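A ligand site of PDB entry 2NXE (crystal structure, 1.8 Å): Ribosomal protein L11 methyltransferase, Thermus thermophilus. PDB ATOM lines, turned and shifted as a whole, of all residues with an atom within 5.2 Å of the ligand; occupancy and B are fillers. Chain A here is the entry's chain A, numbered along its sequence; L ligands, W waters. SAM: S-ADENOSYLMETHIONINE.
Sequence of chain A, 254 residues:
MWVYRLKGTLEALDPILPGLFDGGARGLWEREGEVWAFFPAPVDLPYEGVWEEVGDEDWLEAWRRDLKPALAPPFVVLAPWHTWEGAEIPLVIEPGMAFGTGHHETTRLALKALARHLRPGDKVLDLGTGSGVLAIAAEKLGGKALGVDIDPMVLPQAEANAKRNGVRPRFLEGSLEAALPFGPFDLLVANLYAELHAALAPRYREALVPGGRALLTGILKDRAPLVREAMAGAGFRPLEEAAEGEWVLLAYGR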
ATOM      1  N   GLU A  32      -6.555  29.614 -18.561  1.00  0.00           N
ATOM      2  CA  GLU A  32      -5.659  28.745 -19.359  1.00  0.00           C
ATOM      3  C   GLU A  32      -5.114  29.583 -20.497  1.00  0.00           C
ATOM      4  O   GLU A  32      -5.813  29.841 -21.462  1.00  0.00           O
ATOM      5  CB  GLU A  32      -6.446  27.535 -19.880  1.00  0.00           C
ATOM      6  CG  GLU A  32      -5.709  26.561 -20.776  1.00  0.00           C
ATOM      7  CD  GLU A  32      -6.622  25.470 -21.282  1.00  0.00           C
ATOM      8  OE1 GLU A  32      -7.791  25.766 -21.672  1.00  0.00           O
ATOM      9  OE2 GLU A  32      -6.201  24.319 -21.250  1.00  0.00           O
ATOM     10  N   PHE A  99      -3.676  23.137 -16.733  1.00  0.00           N
ATOM     11  CA  PHE A  99      -3.668  23.467 -18.159  1.00  0.00           C
ATOM     12  C   PHE A  99      -3.890  22.191 -18.965  1.00  0.00           C
ATOM     13  O   PHE A  99      -3.331  21.153 -18.652  1.00  0.00           O
ATOM     14  CB  PHE A  99      -2.307  24.051 -18.501  1.00  0.00           C
ATOM     15  CG  PHE A  99      -2.246  24.817 -19.790  1.00  0.00           C
ATOM     16  CD1 PHE A  99      -2.366  24.155 -21.032  1.00  0.00           C
ATOM     17  CD2 PHE A  99      -2.048  26.203 -19.789  1.00  0.00           C
ATOM     18  CE1 PHE A  99      -2.256  24.862 -22.247  1.00  0.00           C
ATOM     19  CE2 PHE A  99      -1.963  26.899 -20.991  1.00  0.00           C
ATOM     20  CZ  PHE A  99      -2.074  26.219 -22.231  1.00  0.00           C
ATOM     21  N   GLY A 100      -4.716  22.295 -20.004  1.00  0.00           N
ATOM     22  CA  GLY A 100      -5.005  21.169 -20.891  1.00  0.00           C
ATOM     23  C   GLY A 100      -6.472  20.768 -21.001  1.00  0.00           C
ATOM     24  O   GLY A 100      -6.809  19.568 -21.055  1.00  0.00           O
ATOM     25  N   THR A 106      -2.262  25.363 -28.335  1.00  0.00           N
ATOM     26  CA  THR A 106      -1.038  24.575 -28.153  1.00  0.00           C
ATOM     27  C   THR A 106      -1.364  23.090 -27.892  1.00  0.00           C
ATOM     28  O   THR A 106      -0.740  22.182 -28.477  1.00  0.00           O
ATOM     29  CB  THR A 106      -0.164  25.165 -27.033  1.00  0.00           C
ATOM     30  OG1 THR A 106      -0.884  25.151 -25.798  1.00  0.00           O
ATOM     31  CG2 THR A 106       0.274  26.601 -27.423  1.00  0.00           C
ATOM     32  N   THR A 107      -2.338  22.857 -27.020  1.00  0.00           N
ATOM     33  CA  THR A 107      -2.825  21.513 -26.703  1.00  0.00           C
ATOM     34  C   THR A 107      -3.307  20.814 -27.963  1.00  0.00           C
ATOM     35  O   THR A 107      -2.985  19.634 -28.206  1.00  0.00           O
ATOM     36  CB  THR A 107      -3.987  21.607 -25.673  1.00  0.00           C
ATOM     37  OG1 THR A 107      -3.567  22.407 -24.549  1.00  0.00           O
ATOM     38  CG2 THR A 107      -4.383  20.232 -25.194  1.00  0.00           C
ATOM     39  N   ALA A 110      -0.498  19.884 -30.293  1.00  0.00           N
ATOM     40  CA  ALA A 110       0.145  18.698 -29.740  1.00  0.00           C
ATOM     41  C   ALA A 110      -0.646  17.421 -30.010  1.00  0.00           C
ATOM     42  O   ALA A 110      -0.069  16.404 -30.371  1.00  0.00           O
ATOM     43  CB  ALA A 110       0.378  18.895 -28.249  1.00  0.00           C
ATOM     44  N   ASP A 126       5.149  12.538 -21.995  1.00  0.00           N
ATOM     45  CA  ASP A 126       4.344  13.780 -22.006  1.00  0.00           C
ATOM     46  C   ASP A 126       4.950  14.662 -20.919  1.00  0.00           C
ATOM     47  O   ASP A 126       4.617  14.522 -19.752  1.00  0.00           O
ATOM     48  CB  ASP A 126       2.859  13.438 -21.761  1.00  0.00           C
ATOM     49  CG  ASP A 126       1.939  14.677 -21.596  1.00  0.00           C
ATOM     50  OD1 ASP A 126       2.340  15.788 -21.971  1.00  0.00           O
ATOM     51  OD2 ASP A 126       0.798  14.518 -21.100  1.00  0.00           O
ATOM     52  N   LEU A 127       5.818  15.589 -21.322  1.00  0.00           N
ATOM     53  CA  LEU A 127       6.542  16.455 -20.397  1.00  0.00           C
ATOM     54  C   LEU A 127       5.745  17.723 -20.175  1.00  0.00           C
ATOM     55  O   LEU A 127       5.507  18.506 -21.114  1.00  0.00           O
ATOM     56  CB  LEU A 127       7.938  16.792 -20.949  1.00  0.00           C
ATOM     57  CG  LEU A 127       8.894  17.689 -20.130  1.00  0.00           C
ATOM     58  CD1 LEU A 127       9.253  17.056 -18.793  1.00  0.00           C
ATOM     59  CD2 LEU A 127      10.160  17.938 -20.973  1.00  0.00           C
ATOM     60  N   GLY A 128       5.304  17.883 -18.927  1.00  0.00           N
ATOM     61  CA  GLY A 128       4.388  18.946 -18.539  1.00  0.00           C
ATOM     62  C   GLY A 128       2.940  18.527 -18.817  1.00  0.00           C
ATOM     63  O   GLY A 128       2.234  19.150 -19.634  1.00  0.00           O
ATOM     64  N   THR A 129       2.512  17.452 -18.176  1.00  0.00           N
ATOM     65  CA  THR A 129       1.260  16.798 -18.496  1.00  0.00           C
ATOM     66  C   THR A 129      -0.012  17.580 -18.174  1.00  0.00           C
ATOM     67  O   THR A 129      -1.030  17.397 -18.854  1.00  0.00           O
ATOM     68  CB  THR A 129       1.222  15.387 -17.923  1.00  0.00           C
ATOM     69  OG1 THR A 129       0.248  14.593 -18.619  1.00  0.00           O
ATOM     70  CG2 THR A 129       0.974  15.386 -16.417  1.00  0.00           C
ATOM     71  N   GLY A 130       0.031  18.460 -17.171  1.00  0.00           N
ATOM     72  CA  GLY A 130      -1.180  19.158 -16.749  1.00  0.00           C
ATOM     73  C   GLY A 130      -2.383  18.257 -16.547  1.00  0.00           C
ATOM     74  O   GLY A 130      -2.344  17.359 -15.723  1.00  0.00           O
ATOM     75  N   SER A 131      -3.468  18.489 -17.304  1.00  0.00           N
ATOM     76  CA  SER A 131      -4.713  17.707 -17.162  1.00  0.00           C
ATOM     77  C   SER A 131      -4.530  16.220 -17.511  1.00  0.00           C
ATOM     78  O   SER A 131      -5.449  15.430 -17.292  1.00  0.00           O
ATOM     79  CB  SER A 131      -5.758  18.256 -18.151  1.00  0.00           C
ATOM     80  OG  SER A 131      -5.255  18.031 -19.449  1.00  0.00           O
ATOM     81  N   VAL A 133      -4.192  15.252 -20.673  1.00  0.00           N
ATOM     82  CA  VAL A 133      -4.815  15.005 -21.959  1.00  0.00           C
ATOM     83  C   VAL A 133      -3.887  14.346 -23.024  1.00  0.00           C
ATOM     84  O   VAL A 133      -4.329  13.441 -23.747  1.00  0.00           O
ATOM     85  CB  VAL A 133      -5.575  16.287 -22.450  1.00  0.00           C
ATOM     86  CG1 VAL A 133      -4.599  17.467 -22.565  1.00  0.00           C
ATOM     87  CG2 VAL A 133      -6.318  16.016 -23.761  1.00  0.00           C
ATOM     88  N   LEU A 134      -2.619  14.769 -23.110  1.00  0.00           N
ATOM     89  CA  LEU A 134      -1.722  14.229 -24.162  1.00  0.00           C
ATOM     90  C   LEU A 134      -1.351  12.771 -23.862  1.00  0.00           C
ATOM     91  O   LEU A 134      -1.348  11.922 -24.768  1.00  0.00           O
ATOM     92  CB  LEU A 134      -0.509  15.099 -24.392  1.00  0.00           C
ATOM     93  CG  LEU A 134      -0.758  16.554 -24.737  1.00  0.00           C
ATOM     94  CD1 LEU A 134       0.536  17.349 -24.989  1.00  0.00           C
ATOM     95  CD2 LEU A 134      -1.732  16.706 -25.944  1.00  0.00           C
ATOM     96  N   VAL A 148       4.466  13.656 -16.792  1.00  0.00           N
ATOM     97  CA  VAL A 148       5.124  14.207 -15.612  1.00  0.00           C
ATOM     98  C   VAL A 148       4.838  15.684 -15.553  1.00  0.00           C
ATOM     99  O   VAL A 148       4.638  16.321 -16.587  1.00  0.00           O
ATOM    100  CB  VAL A 148       6.693  13.886 -15.566  1.00  0.00           C
ATOM    101  CG1 VAL A 148       6.966  12.403 -15.851  1.00  0.00           C
ATOM    102  CG2 VAL A 148       7.453  14.749 -16.561  1.00  0.00           C
ATOM    103  N   ASP A 149       4.765  16.233 -14.340  1.00  0.00           N
ATOM    104  CA  ASP A 149       4.534  17.658 -14.165  1.00  0.00           C
ATOM    105  C   ASP A 149       5.194  18.120 -12.885  1.00  0.00           C
ATOM    106  O   ASP A 149       5.180  17.405 -11.870  1.00  0.00           O
ATOM    107  CB  ASP A 149       3.048  17.976 -14.065  1.00  0.00           C
ATOM    108  CG  ASP A 149       2.721  19.412 -14.464  1.00  0.00           C
ATOM    109  OD1 ASP A 149       2.114  19.602 -15.543  1.00  0.00           O
ATOM    110  OD2 ASP A 149       3.034  20.370 -13.717  1.00  0.00           O
ATOM    111  N   ILE A 150       5.773  19.321 -12.944  1.00  0.00           N
ATOM    112  CA  ILE A 150       6.426  19.871 -11.752  1.00  0.00           C
ATOM    113  C   ILE A 150       5.448  20.373 -10.703  1.00  0.00           C
ATOM    114  O   ILE A 150       5.856  20.671  -9.571  1.00  0.00           O
ATOM    115  CB  ILE A 150       7.485  20.973 -12.054  1.00  0.00           C
ATOM    116  CG1 ILE A 150       6.861  22.109 -12.876  1.00  0.00           C
ATOM    117  CG2 ILE A 150       8.744  20.346 -12.656  1.00  0.00           C
ATOM    118  CD1 ILE A 150       7.573  23.453 -12.782  1.00  0.00           C
ATOM    119  N   ASP A 151       4.189  20.483 -11.096  1.00  0.00           N
ATOM    120  CA  ASP A 151       3.133  20.890 -10.190  1.00  0.00           C
ATOM    121  C   ASP A 151       2.378  19.632  -9.763  1.00  0.00           C
ATOM    122  O   ASP A 151       1.546  19.142 -10.518  1.00  0.00           O
ATOM    123  CB  ASP A 151       2.173  21.897 -10.862  1.00  0.00           C
ATOM    124  CG  ASP A 151       1.132  22.426  -9.918  1.00  0.00           C
ATOM    125  OD1 ASP A 151       1.138  22.013  -8.728  1.00  0.00           O
ATOM    126  OD2 ASP A 151       0.309  23.276 -10.346  1.00  0.00           O
ATOM    127  N   VAL A 154      -1.530  18.881 -10.179  1.00  0.00           N
ATOM    128  CA  VAL A 154      -2.261  18.501 -11.410  1.00  0.00           C
ATOM    129  C   VAL A 154      -2.486  16.992 -11.424  1.00  0.00           C
ATOM    130  O   VAL A 154      -3.323  16.469 -12.145  1.00  0.00           O
ATOM    131  CB  VAL A 154      -1.474  18.917 -12.702  1.00  0.00           C
ATOM    132  CG1 VAL A 154      -1.129  20.413 -12.720  1.00  0.00           C
ATOM    133  CG2 VAL A 154      -0.208  18.079 -12.887  1.00  0.00           C
ATOM    134  N   GLY A 174       7.495  15.652 -11.320  1.00  0.00           N
ATOM    135  CA  GLY A 174       8.888  15.895 -11.690  1.00  0.00           C
ATOM    136  C   GLY A 174       9.035  16.505 -13.058  1.00  0.00           C
ATOM    137  O   GLY A 174       8.049  16.928 -13.694  1.00  0.00           O
ATOM    138  N   SER A 175      10.282  16.539 -13.516  1.00  0.00           N
ATOM    139  CA  SER A 175      10.562  17.027 -14.835  1.00  0.00           C
ATOM    140  C   SER A 175      11.239  15.954 -15.670  1.00  0.00           C
ATOM    141  O   SER A 175      11.084  14.758 -15.398  1.00  0.00           O
ATOM    142  CB  SER A 175      11.364  18.310 -14.780  1.00  0.00           C
ATOM    143  OG  SER A 175      11.365  18.928 -16.050  1.00  0.00           O
ATOM    144  N   LEU A 176      11.979  16.373 -16.692  1.00  0.00           N
ATOM    145  CA  LEU A 176      12.621  15.433 -17.583  1.00  0.00           C
ATOM    146  C   LEU A 176      13.473  14.446 -16.777  1.00  0.00           C
ATOM    147  O   LEU A 176      13.505  13.259 -17.084  1.00  0.00           O
ATOM    148  CB  LEU A 176      13.448  16.199 -18.643  1.00  0.00           C
ATOM    149  CG  LEU A 176      14.070  15.454 -19.823  1.00  0.00           C
ATOM    150  CD1 LEU A 176      13.113  14.450 -20.491  1.00  0.00           C
ATOM    151  CD2 LEU A 176      14.607  16.456 -20.838  1.00  0.00           C
ATOM    152  N   ASN A 191       4.461  20.391 -24.395  1.00  0.00           N
ATOM    153  CA  ASN A 191       3.807  21.690 -24.534  1.00  0.00           C
ATOM    154  C   ASN A 191       4.299  22.537 -23.395  1.00  0.00           C
ATOM    155  O   ASN A 191       3.696  22.518 -22.313  1.00  0.00           O
ATOM    156  CB  ASN A 191       2.285  21.538 -24.448  1.00  0.00           C
ATOM    157  CG  ASN A 191       1.521  22.862 -24.717  1.00  0.00           C
ATOM    158  OD1 ASN A 191       2.136  23.917 -24.971  1.00  0.00           O
ATOM    159  ND2 ASN A 191       0.194  22.783 -24.680  1.00  0.00           N
ATOM    160  N   LEU A 192       5.388  23.262 -23.616  1.00  0.00           N
ATOM    161  CA  LEU A 192       6.047  24.055 -22.569  1.00  0.00           C
ATOM    162  C   LEU A 192       6.136  25.502 -23.007  1.00  0.00           C
ATOM    163  O   LEU A 192       5.080  26.183 -23.157  1.00  0.00           O
ATOM    164  CB  LEU A 192       7.412  23.453 -22.160  1.00  0.00           C
ATOM    165  CG  LEU A 192       7.316  22.055 -21.524  1.00  0.00           C
ATOM    166  CD1 LEU A 192       8.699  21.383 -21.478  1.00  0.00           C
ATOM    167  CD2 LEU A 192       6.651  22.102 -20.150  1.00  0.00           C
ATOM    168  N   TYR A 193       7.368  25.982 -23.238  1.00  0.00           N
ATOM    169  CA  TYR A 193       7.627  27.336 -23.747  1.00  0.00           C
ATOM    170  C   TYR A 193       9.024  27.368 -24.360  1.00  0.00           C
ATOM    171  O   TYR A 193       9.830  26.495 -24.086  1.00  0.00           O
ATOM    172  CB  TYR A 193       7.437  28.414 -22.666  1.00  0.00           C
ATOM    173  CG  TYR A 193       8.147  28.162 -21.356  1.00  0.00           C
ATOM    174  CD1 TYR A 193       9.405  28.735 -21.092  1.00  0.00           C
ATOM    175  CD2 TYR A 193       7.580  27.355 -20.360  1.00  0.00           C
ATOM    176  CE1 TYR A 193      10.078  28.510 -19.885  1.00  0.00           C
ATOM    177  CE2 TYR A 193       8.235  27.123 -19.144  1.00  0.00           C
ATOM    178  CZ  TYR A 193       9.487  27.701 -18.913  1.00  0.00           C
ATOM    179  OH  TYR A 193      10.133  27.484 -17.730  1.00  0.00           O
ATOM    180  N   LEU A 196      12.511  27.068 -22.397  1.00  0.00           N
ATOM    181  CA  LEU A 196      12.717  25.814 -21.726  1.00  0.00           C
ATOM    182  C   LEU A 196      13.073  24.679 -22.688  1.00  0.00           C
ATOM    183  O   LEU A 196      13.952  23.899 -22.378  1.00  0.00           O
ATOM    184  CB  LEU A 196      11.518  25.458 -20.813  1.00  0.00           C
ATOM    185  CG  LEU A 196      11.530  24.103 -20.141  1.00  0.00           C
ATOM    186  CD1 LEU A 196      12.708  23.957 -19.168  1.00  0.00           C
ATOM    187  CD2 LEU A 196      10.217  23.921 -19.409  1.00  0.00           C
HETATM  188  N   SAM L   1       0.447  18.929 -21.723  1.00  0.00           N
HETATM  189  CA  SAM L   1      -0.766  19.774 -21.374  1.00  0.00           C
HETATM  190  C   SAM L   1      -1.327  20.421 -22.627  1.00  0.00           C
HETATM  191  O   SAM L   1      -0.734  20.249 -23.698  1.00  0.00           O
HETATM  192  OXT SAM L   1      -2.336  21.153 -22.589  1.00  0.00           O
HETATM  193  CB  SAM L   1      -0.353  20.928 -20.453  1.00  0.00           C
HETATM  194  CG  SAM L   1       0.524  22.014 -21.067  1.00  0.00           C
HETATM  195  SD  SAM L   1       0.867  23.439 -19.985  1.00  0.00           S
HETATM  196  CE  SAM L   1       1.260  24.685 -21.210  1.00  0.00           C
HETATM  197  C5' SAM L   1       2.526  23.074 -19.332  1.00  0.00           C
HETATM  198  C4' SAM L   1       2.511  22.204 -18.086  1.00  0.00           C
HETATM  199  O4' SAM L   1       3.897  21.940 -17.832  1.00  0.00           O
HETATM  200  C3' SAM L   1       1.938  22.857 -16.835  1.00  0.00           C
HETATM  201  O3' SAM L   1       1.058  21.936 -16.208  1.00  0.00           O
HETATM  202  C2' SAM L   1       3.179  23.127 -15.965  1.00  0.00           C
HETATM  203  O2' SAM L   1       2.908  23.015 -14.575  1.00  0.00           O
HETATM  204  C1' SAM L   1       4.175  22.081 -16.442  1.00  0.00           C
HETATM  205  N9  SAM L   1       5.598  22.456 -16.397  1.00  0.00           N
HETATM  206  C8  SAM L   1       6.168  23.713 -16.523  1.00  0.00           C
HETATM  207  N7  SAM L   1       7.522  23.569 -16.477  1.00  0.00           N
HETATM  208  C5  SAM L   1       7.816  22.247 -16.340  1.00  0.00           C
HETATM  209  C6  SAM L   1       8.995  21.509 -16.231  1.00  0.00           C
HETATM  210  N6  SAM L   1      10.171  22.135 -16.283  1.00  0.00           N
HETATM  211  N1  SAM L   1       8.948  20.127 -16.114  1.00  0.00           N
HETATM  212  C2  SAM L   1       7.752  19.436 -16.060  1.00  0.00           C
HETATM  213  N3  SAM L   1       6.581  20.178 -16.172  1.00  0.00           N
HETATM  214  C4  SAM L   1       6.613  21.530 -16.298  1.00  0.00           C
HETATM  215  O   HOH W   1       3.197  18.487 -22.619  1.00  0.00           O
HETATM  216  O   HOH W   2      13.012  21.179 -16.191  1.00  0.00           O
HETATM  217  O   HOH W   3       8.976  25.703 -15.995  1.00  0.00           O
HETATM  218  O   HOH W   4       1.306  26.790 -23.894  1.00  0.00           O
HETATM  219  O   HOH W   5      -0.976  16.478 -21.293  1.00  0.00           O
HETATM  220  O   HOH W   6      -1.172  23.257 -15.229  1.00  0.00           O
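O of Asp 149 lies within hydrogen-bond range of N of Gly 174, at 3.0 Å.
N of Gly 130 is in hydrogen-bond range of OD1 of Asp 149, 2.9 Å away.
The side-chain hydroxyl (OG1) of Thr 106 sits at hydrogen-bond distance from the side-chain amide nitrogen (ND2) of Asn 191 (2.8 Å).
The backbone carbonyl oxygen (O) of Gly 100 lies within hydrogen-bond range of the side-chain hydroxyl (OG) of Ser 131, 2.7 Å away.
The backbone NH (N) of Gly 100 sits at hydrogen-bond distance from the side-chain carboxylate (OE2) of Glu 32 (2.8 Å).
N of Ser 131 is in hydrogen-bond range of O of Phe 99, at 3.0 Å.
OD2 of Asp 126 is in hydrogen-bond range of OG1 of Thr 129, 2.5 Å away.
The backbone NH (N) of Thr 129 is in hydrogen-bond range of the backbone carbonyl oxygen (O) of Val 148, 2.9 Å away.
The side-chain hydroxyl of Thr 107 lies within hydrogen-bond range of an oxygen (OXT) of the ligand (2.6 Å).
The side-chain carboxylate of Asp 149 lies within hydrogen-bond range of an oxygen (O3') of the ligand, 2.6 Å away.
The side-chain hydroxyl of Ser 175 is in hydrogen-bond range of a nitrogen (N1) of the ligand, at 2.7 Å.
N of the ligand is in hydrogen-bond range of O of Gly 128, at 2.8 Å.
An oxygen (O) of the ligand lies within hydrogen-bond range of the side-chain amide nitrogen of Asn 191.
The backbone NH (N) of Ile 150 is in hydrogen-bond range of a nitrogen (N3) of the ligand (3.4 Å).
A nitrogen (N) of the ligand is in salt-bridge range of the side-chain carboxylate of Asp 126 (3.7 Å).
Water W3 lies within hydrogen-bond range of a nitrogen (N7) of the ligand and the side-chain hydroxyl (OH) of Tyr 193.
Water W6 bridges O3' of the ligand (2.8 Å) and N of Phe 99 (2.9 Å).
Water W5 lies within hydrogen-bond range of the backbone carbonyl oxygen (O) of Thr 129, the side-chain carboxylate (OD2) of Asp 126, a nitrogen (N) of the ligand, the backbone NH (N) of Leu 134 and the backbone NH (N) of Val 133.
Water W2 bridges the side-chain hydroxyl (OG) of Ser 175 (2.8 Å) and a nitrogen (N6) of the ligand (3.0 Å).
Water W4 bridges the side-chain amide oxygen of Asn 191 (3.2 Å) and the side-chain hydroxyl of Thr 106 (3.3 Å).
CD1 of Phe 99 touches OXT of the ligand, at 3.4 Å.
Gly 100 touches the ligand (CA to OXT, 3.2 Å).
CD1 of Leu 127 touches C2 of the ligand, at 3.9 Å.
Thr 129 touches the ligand.
CA of Gly 130 touches O3' of the ligand, 3.6 Å away.
Leu 134 touches the ligand.
Asp 151 touches the ligand.
Gly 174 touches the ligand.
Leu 192 touches the ligand (CD2 to O4', 3.6 Å).
Leu 196 touches the ligand.
Hydrophobic or aromatic side chains within 4 Å of the ligand: Phe 99, Leu 127, Leu 134, Ile 150, Leu 192 and Leu 196.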
